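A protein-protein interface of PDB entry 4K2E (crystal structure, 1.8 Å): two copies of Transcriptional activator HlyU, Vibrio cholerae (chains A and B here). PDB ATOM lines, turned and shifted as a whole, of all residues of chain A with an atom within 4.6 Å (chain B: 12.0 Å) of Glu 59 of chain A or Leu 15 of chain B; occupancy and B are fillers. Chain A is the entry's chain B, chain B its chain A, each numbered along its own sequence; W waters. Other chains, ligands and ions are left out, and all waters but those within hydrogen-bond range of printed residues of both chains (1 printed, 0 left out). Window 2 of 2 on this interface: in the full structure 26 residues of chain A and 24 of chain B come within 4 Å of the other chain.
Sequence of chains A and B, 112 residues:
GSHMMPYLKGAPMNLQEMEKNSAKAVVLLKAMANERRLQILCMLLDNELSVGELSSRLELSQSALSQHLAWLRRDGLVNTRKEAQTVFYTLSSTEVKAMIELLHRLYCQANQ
OG of Ser 22 of chain B is in hydrogen-bond range of NE2 of Gln 39 of chain A (3.1 Å).
The side-chain carboxylate (OE2) of Glu 19 of chain B is in salt-bridge range of the guanidinium group (NH2) of Arg 36 of chain A (3.7 Å).
O of Leu 58 of chain A is in hydrogen-bond range of NH1 of Arg 36 of chain A (2.7 Å).
The side-chain hydroxyl (OG) of Ser 22 of chain B is in hydrogen-bond range of the backbone carbonyl oxygen (O) of Glu 19 of chain B (3.0 Å).
The backbone carbonyl oxygen of Met 18 of chain B lies within hydrogen-bond range of the side-chain hydroxyl of Ser 22 of chain B (2.9 Å).
OE1 of Gln 39 of chain A is in hydrogen-bond range of NH1 of Arg 36 of chain A.
The side-chain carboxylate (OE2) of Glu 17 of chain B is in hydrogen-bond range of the backbone NH (N) of Leu 15 of chain B, 2.7 Å away.
CD1 of Leu 15 of chain B touches NH1 of Arg 36 of chain A, 3.9 Å away.
Gln 39 of chain A touches Leu 15 of chain B (OE1 to CD1, 3.8 Å).
CG of Gln 39 of chain A touches CG of Met 18 of chain B, 3.6 Å away.
Glu 19 of chain B touches Gln 39 of chain A (CG to NE2, 3.5 Å).
Arg 57 of chain A touches Leu 15 of chain B (O to CB, 3.8 Å).
Leu 58 of chain A touches Leu 15 of chain B.
Glu 59 of chain A touches Leu 15 of chain B.
Glu 59 of chain A touches just one residue of chain B: Leu 15.
Of chain A, only Arg 36 (3.9 Å), Gln 39 (3.8 Å), Arg 57 (3.8 Å), Leu 58 (3.5 Å) and Glu 59 (3.8 Å) come within 4 Å of Leu 15 of chain B.
No residue of chain B comes within 4 Å of Ser 55 of chain A.
Ser 56 of chain A touches none of the printed residues of chain B.
Printed residues of chain B within 4 Å of Leu 58 of chain A: Leu 15 (3.5 Å).
No residue of chain B comes within 4 Å of Ser 61 of chain A.
Printed residues of chain A within 4 Å of Glu 19 of chain B: Arg 36 and Gln 39.
Of the printed residues of chain A, Ser 22 of chain B touches Gln 39 (3.1 Å).
Of the printed residues of chain B, Arg 36 of chain A touches Leu 15 (3.9 Å) and Glu 19 (3.7 Å).
Of the printed residues of chain B, Gln 39 of chain A touches Leu 15 (3.8 Å), Met 18 (3.6 Å), Glu 19 (3.5 Å) and Ser 22 (3.1 Å).
Val 26 of chain B touches none of the printed residues of chain A.
The nearest printed residue of chain A that does not touch Leu 15 of chain B is Ser 56 of chain A (6.4 Å).
The nearest printed residue of chain A that does not touch Glu 19 of chain B is Leu 58 of chain A (5.7 Å).
Printed residues of chain A that touch a printed residue of chain B: Arg 36, Gln 39, Arg 57, Leu 58 and Glu 59.
Hydrophobic or aromatic side chains of chain B within 4 Å of the printed part of chain A: Leu 15 and Met 18.
Along chain B the printed residues that touch a printed residue of chain A span positions 15 to 22.
Among the printed residues, 9 pairs touch across the chains.
Among the printed residues, Asp or Glu carboxylates within 4 Å of a Lys or Arg side-chain nitrogen of the other chain: Arg 36 of chain A with Glu 19 of chain B.
No position is printed for both chains.
Of the 9 pairs that touch across the chains among the printed residues, none has its exchanged pair printed and touching as well.
Water W1 lies within hydrogen-bond range of the side-chain carboxylate of Glu 19 of chain B (2.6 Å), the side-chain amide nitrogen of Gln 39 of chain A (3.1 Å) and the guanidinium group of Arg 36 of chain A (3.4 Å).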
ATOM      1  N   ARG A  36       6.112  -4.666 -23.848  1.00  0.00           N
ATOM      2  CA  ARG A  36       5.575  -6.014 -24.106  1.00  0.00           C
ATOM      3  C   ARG A  36       4.938  -6.627 -22.855  1.00  0.00           C
ATOM      4  O   ARG A  36       3.825  -7.183 -22.919  1.00  0.00           O
ATOM      5  CB  ARG A  36       6.627  -6.941 -24.695  1.00  0.00           C
ATOM      6  CG  ARG A  36       7.047  -6.523 -26.086  1.00  0.00           C
ATOM      7  CD  ARG A  36       5.833  -6.412 -26.979  1.00  0.00           C
ATOM      8  NE  ARG A  36       6.203  -6.337 -28.378  1.00  0.00           N
ATOM      9  CZ  ARG A  36       5.384  -6.683 -29.380  1.00  0.00           C
ATOM     10  NH1 ARG A  36       4.148  -7.100 -29.110  1.00  0.00           N
ATOM     11  NH2 ARG A  36       5.785  -6.607 -30.648  1.00  0.00           N
ATOM     12  N   GLN A  39       1.624  -4.974 -22.326  1.00  0.00           N
ATOM     13  CA  GLN A  39       0.664  -5.465 -23.327  1.00  0.00           C
ATOM     14  C   GLN A  39       0.062  -6.811 -22.922  1.00  0.00           C
ATOM     15  O   GLN A  39      -1.173  -7.025 -23.025  1.00  0.00           O
ATOM     16  CB  GLN A  39       1.353  -5.592 -24.685  1.00  0.00           C
ATOM     17  CG  GLN A  39       1.612  -4.259 -25.326  1.00  0.00           C
ATOM     18  CD  GLN A  39       2.501  -4.346 -26.547  1.00  0.00           C
ATOM     19  OE1 GLN A  39       2.688  -5.419 -27.127  1.00  0.00           O
ATOM     20  NE2 GLN A  39       3.066  -3.209 -26.936  1.00  0.00           N
ATOM     21  N   SER A  55       0.876 -14.994 -28.250  1.00  0.00           N
ATOM     22  CA  SER A  55       1.902 -14.787 -29.273  1.00  0.00           C
ATOM     23  C   SER A  55       1.297 -14.325 -30.584  1.00  0.00           C
ATOM     24  O   SER A  55       1.847 -13.462 -31.276  1.00  0.00           O
ATOM     25  CB  SER A  55       2.793 -16.029 -29.452  1.00  0.00           C
ATOM     26  OG  SER A  55       2.057 -17.181 -29.832  1.00  0.00           O
ATOM     27  N   SER A  56       0.141 -14.897 -30.905  1.00  0.00           N
ATOM     28  CA  SER A  56      -0.577 -14.513 -32.084  1.00  0.00           C
ATOM     29  C   SER A  56      -0.961 -13.042 -32.064  1.00  0.00           C
ATOM     30  O   SER A  56      -0.774 -12.333 -33.053  1.00  0.00           O
ATOM     31  CB  SER A  56      -1.821 -15.383 -32.259  1.00  0.00           C
ATOM     32  OG  SER A  56      -2.453 -15.036 -33.465  1.00  0.00           O
ATOM     33  N   ARG A  57      -1.515 -12.579 -30.957  1.00  0.00           N
ATOM     34  CA  ARG A  57      -1.938 -11.178 -30.894  1.00  0.00           C
ATOM     35  C   ARG A  57      -0.761 -10.195 -30.795  1.00  0.00           C
ATOM     36  O   ARG A  57      -0.809  -9.101 -31.339  1.00  0.00           O
ATOM     37  CB  ARG A  57      -2.945 -10.977 -29.752  1.00  0.00           C
ATOM     38  CG  ARG A  57      -4.361 -11.384 -30.185  1.00  0.00           C
ATOM     39  CD  ARG A  57      -5.311 -11.620 -29.020  1.00  0.00           C
ATOM     40  NE  ARG A  57      -5.691 -10.388 -28.337  1.00  0.00           N
ATOM     41  CZ  ARG A  57      -6.532 -10.337 -27.306  1.00  0.00           C
ATOM     42  NH1 ARG A  57      -7.090 -11.453 -26.846  1.00  0.00           N
ATOM     43  NH2 ARG A  57      -6.818  -9.176 -26.734  1.00  0.00           N
ATOM     44  N   LEU A  58       0.302 -10.608 -30.117  1.00  0.00           N
ATOM     45  CA  LEU A  58       1.455  -9.743 -29.863  1.00  0.00           C
ATOM     46  C   LEU A  58       2.443  -9.713 -31.018  1.00  0.00           C
ATOM     47  O   LEU A  58       3.290  -8.799 -31.091  1.00  0.00           O
ATOM     48  CB  LEU A  58       2.173 -10.198 -28.584  1.00  0.00           C
ATOM     49  CG  LEU A  58       1.351 -10.062 -27.307  1.00  0.00           C
ATOM     50  CD1 LEU A  58       1.761 -11.106 -26.293  1.00  0.00           C
ATOM     51  CD2 LEU A  58       1.548  -8.686 -26.698  1.00  0.00           C
ATOM     52  N   GLU A  59       2.331 -10.680 -31.936  1.00  0.00           N
ATOM     53  CA  GLU A  59       3.319 -10.841 -33.011  1.00  0.00           C
ATOM     54  C   GLU A  59       4.762 -10.949 -32.476  1.00  0.00           C
ATOM     55  O   GLU A  59       5.676 -10.238 -32.925  1.00  0.00           O
ATOM     56  CB  GLU A  59       3.196  -9.738 -34.068  1.00  0.00           C
ATOM     57  CG  GLU A  59       1.875  -9.759 -34.801  1.00  0.00           C
ATOM     58  CD  GLU A  59       1.728  -8.609 -35.779  1.00  0.00           C
ATOM     59  OE1 GLU A  59       2.728  -7.905 -36.061  1.00  0.00           O
ATOM     60  OE2 GLU A  59       0.596  -8.403 -36.251  1.00  0.00           O
ATOM     61  N   LEU A  60       4.936 -11.862 -31.528  1.00  0.00           N
ATOM     62  CA  LEU A  60       6.251 -12.226 -31.000  1.00  0.00           C
ATOM     63  C   LEU A  60       6.497 -13.706 -31.239  1.00  0.00           C
ATOM     64  O   LEU A  60       5.546 -14.499 -31.262  1.00  0.00           O
ATOM     65  CB  LEU A  60       6.299 -11.998 -29.494  1.00  0.00           C
ATOM     66  CG  LEU A  60       6.251 -10.563 -28.995  1.00  0.00           C
ATOM     67  CD1 LEU A  60       6.195 -10.564 -27.460  1.00  0.00           C
ATOM     68  CD2 LEU A  60       7.452  -9.732 -29.514  1.00  0.00           C
ATOM     69  N   SER A  61       7.766 -14.079 -31.391  1.00  0.00           N
ATOM     70  CA  SER A  61       8.134 -15.490 -31.400  1.00  0.00           C
ATOM     71  C   SER A  61       7.737 -16.040 -30.031  1.00  0.00           C
ATOM     72  O   SER A  61       7.591 -15.286 -29.047  1.00  0.00           O
ATOM     73  CB  SER A  61       9.631 -15.653 -31.588  1.00  0.00           C
ATOM     74  OG  SER A  61      10.258 -15.287 -30.375  1.00  0.00           O
ATOM     75  N   LEU B  15      -3.072  -4.335 -32.204  1.00  0.00           N
ATOM     76  CA  LEU B  15      -1.735  -4.368 -31.622  1.00  0.00           C
ATOM     77  C   LEU B  15      -1.060  -3.003 -31.703  1.00  0.00           C
ATOM     78  O   LEU B  15      -0.408  -2.579 -30.759  1.00  0.00           O
ATOM     79  CB  LEU B  15      -0.859  -5.422 -32.308  1.00  0.00           C
ATOM     80  CG  LEU B  15       0.632  -5.368 -31.937  1.00  0.00           C
ATOM     81  CD1 LEU B  15       0.847  -5.602 -30.451  1.00  0.00           C
ATOM     82  CD2 LEU B  15       1.451  -6.349 -32.755  1.00  0.00           C
ATOM     83  N   GLN B  16      -1.215  -2.321 -32.836  1.00  0.00           N
ATOM     84  CA  GLN B  16      -0.564  -1.024 -33.038  1.00  0.00           C
ATOM     85  C   GLN B  16      -1.003   0.047 -32.034  1.00  0.00           C
ATOM     86  O   GLN B  16      -0.161   0.742 -31.462  1.00  0.00           O
ATOM     87  CB  GLN B  16      -0.760  -0.529 -34.469  1.00  0.00           C
ATOM     88  CG  GLN B  16       0.164  -1.186 -35.485  1.00  0.00           C
ATOM     89  CD  GLN B  16      -0.161  -2.649 -35.737  1.00  0.00           C
ATOM     90  OE1 GLN B  16      -1.324  -3.023 -35.904  1.00  0.00           O
ATOM     91  NE2 GLN B  16       0.872  -3.485 -35.771  1.00  0.00           N
ATOM     92  N   GLU B  17      -2.310   0.180 -31.824  1.00  0.00           N
ATOM     93  CA  GLU B  17      -2.855   1.152 -30.871  1.00  0.00           C
ATOM     94  C   GLU B  17      -2.445   0.785 -29.453  1.00  0.00           C
ATOM     95  O   GLU B  17      -2.158   1.660 -28.618  1.00  0.00           O
ATOM     96  CB  GLU B  17      -4.386   1.234 -30.987  1.00  0.00           C
ATOM     97  CG  GLU B  17      -5.158  -0.046 -30.629  1.00  0.00           C
ATOM     98  CD  GLU B  17      -4.922  -1.199 -31.602  1.00  0.00           C
ATOM     99  OE1 GLU B  17      -5.446  -1.160 -32.738  1.00  0.00           O
ATOM    100  OE2 GLU B  17      -4.205  -2.150 -31.221  1.00  0.00           O
ATOM    101  N   MET B  18      -2.409  -0.518 -29.189  1.00  0.00           N
ATOM    102  CA  MET B  18      -1.921  -1.033 -27.922  1.00  0.00           C
ATOM    103  C   MET B  18      -0.451  -0.668 -27.754  1.00  0.00           C
ATOM    104  O   MET B  18      -0.013  -0.397 -26.645  1.00  0.00           O
ATOM    105  CB  MET B  18      -2.128  -2.551 -27.826  1.00  0.00           C
ATOM    106  CG  MET B  18      -1.619  -3.152 -26.510  1.00  0.00           C
ATOM    107  SD  MET B  18      -1.952  -4.920 -26.300  1.00  0.00           S
ATOM    108  CE  MET B  18      -2.200  -5.424 -28.000  1.00  0.00           C
ATOM    109  N   GLU B  19       0.306  -0.638 -28.852  1.00  0.00           N
ATOM    110  CA  GLU B  19       1.710  -0.220 -28.769  1.00  0.00           C
ATOM    111  C   GLU B  19       1.812   1.294 -28.498  1.00  0.00           C
ATOM    112  O   GLU B  19       2.629   1.755 -27.676  1.00  0.00           O
ATOM    113  CB  GLU B  19       2.482  -0.629 -30.033  1.00  0.00           C
ATOM    114  CG  GLU B  19       2.620  -2.152 -30.227  1.00  0.00           C
ATOM    115  CD  GLU B  19       3.471  -2.534 -31.438  1.00  0.00           C
ATOM    116  OE1 GLU B  19       3.107  -2.157 -32.576  1.00  0.00           O
ATOM    117  OE2 GLU B  19       4.498  -3.224 -31.253  1.00  0.00           O
ATOM    118  N   LYS B  20       0.949   2.048 -29.179  1.00  0.00           N
ATOM    119  CA  LYS B  20       0.846   3.499 -29.060  1.00  0.00           C
ATOM    120  C   LYS B  20       0.584   3.936 -27.612  1.00  0.00           C
ATOM    121  O   LYS B  20       1.232   4.849 -27.087  1.00  0.00           O
ATOM    122  CB  LYS B  20      -0.276   3.997 -29.979  1.00  0.00           C
ATOM    123  CG  LYS B  20      -0.390   5.509 -30.050  1.00  0.00           C
ATOM    124  CD  LYS B  20      -1.457   5.970 -31.043  1.00  0.00           C
ATOM    125  CE  LYS B  20      -2.861   5.800 -30.488  1.00  0.00           C
ATOM    126  NZ  LYS B  20      -3.868   6.476 -31.356  1.00  0.00           N
ATOM    127  N   ASN B  21      -0.361   3.269 -26.963  1.00  0.00           N
ATOM    128  CA  ASN B  21      -0.699   3.601 -25.590  1.00  0.00           C
ATOM    129  C   ASN B  21       0.269   2.998 -24.578  1.00  0.00           C
ATOM    130  O   ASN B  21       0.600   3.632 -23.557  1.00  0.00           O
ATOM    131  CB  ASN B  21      -2.131   3.152 -25.299  1.00  0.00           C
ATOM    132  CG  ASN B  21      -3.131   3.776 -26.239  1.00  0.00           C
ATOM    133  OD1 ASN B  21      -3.063   4.968 -26.524  1.00  0.00           O
ATOM    134  ND2 ASN B  21      -4.059   2.966 -26.744  1.00  0.00           N
ATOM    135  N   SER B  22       0.713   1.770 -24.865  1.00  0.00           N
ATOM    136  CA  SER B  22       1.640   1.094 -23.975  1.00  0.00           C
ATOM    137  C   SER B  22       2.902   1.923 -23.824  1.00  0.00           C
ATOM    138  O   SER B  22       3.375   2.070 -22.724  1.00  0.00           O
ATOM    139  CB  SER B  22       1.961  -0.352 -24.392  1.00  0.00           C
ATOM    140  OG  SER B  22       2.662  -0.422 -25.622  1.00  0.00           O
ATOM    141  N   ALA B  23       3.408   2.513 -24.906  1.00  0.00           N
ATOM    142  CA  ALA B  23       4.577   3.402 -24.795  1.00  0.00           C
ATOM    143  C   ALA B  23       4.446   4.567 -23.764  1.00  0.00           C
ATOM    144  O   ALA B  23       5.341   4.790 -22.922  1.00  0.00           O
ATOM    145  CB  ALA B  23       4.962   3.930 -26.170  1.00  0.00           C
ATOM    146  N   LYS B  24       3.347   5.317 -23.832  1.00  0.00           N
ATOM    147  CA  LYS B  24       3.152   6.455 -22.927  1.00  0.00           C
ATOM    148  C   LYS B  24       2.965   6.005 -21.473  1.00  0.00           C
ATOM    149  O   LYS B  24       3.557   6.567 -20.500  1.00  0.00           O
ATOM    150  CB  LYS B  24       1.941   7.280 -23.362  1.00  0.00           C
ATOM    151  CG  LYS B  24       1.608   8.443 -22.422  1.00  0.00           C
ATOM    152  CD  LYS B  24       0.538   9.363 -23.024  1.00  0.00           C
ATOM    153  CE  LYS B  24       0.211  10.537 -22.093  1.00  0.00           C
ATOM    154  NZ  LYS B  24      -1.082  11.213 -22.452  1.00  0.00           N
ATOM    155  N   VAL B  26       4.154   3.431 -20.330  1.00  0.00           N
ATOM    156  CA  VAL B  26       5.422   2.878 -19.891  1.00  0.00           C
ATOM    157  C   VAL B  26       6.384   4.000 -19.454  1.00  0.00           C
ATOM    158  O   VAL B  26       7.156   3.821 -18.524  1.00  0.00           O
ATOM    159  CB  VAL B  26       6.051   1.959 -20.958  1.00  0.00           C
ATOM    160  CG1 VAL B  26       7.495   1.680 -20.658  1.00  0.00           C
ATOM    161  CG2 VAL B  26       5.281   0.616 -21.025  1.00  0.00           C
HETATM  162  O   HOH W   1       5.483  -3.018 -28.903  1.00  0.00           O
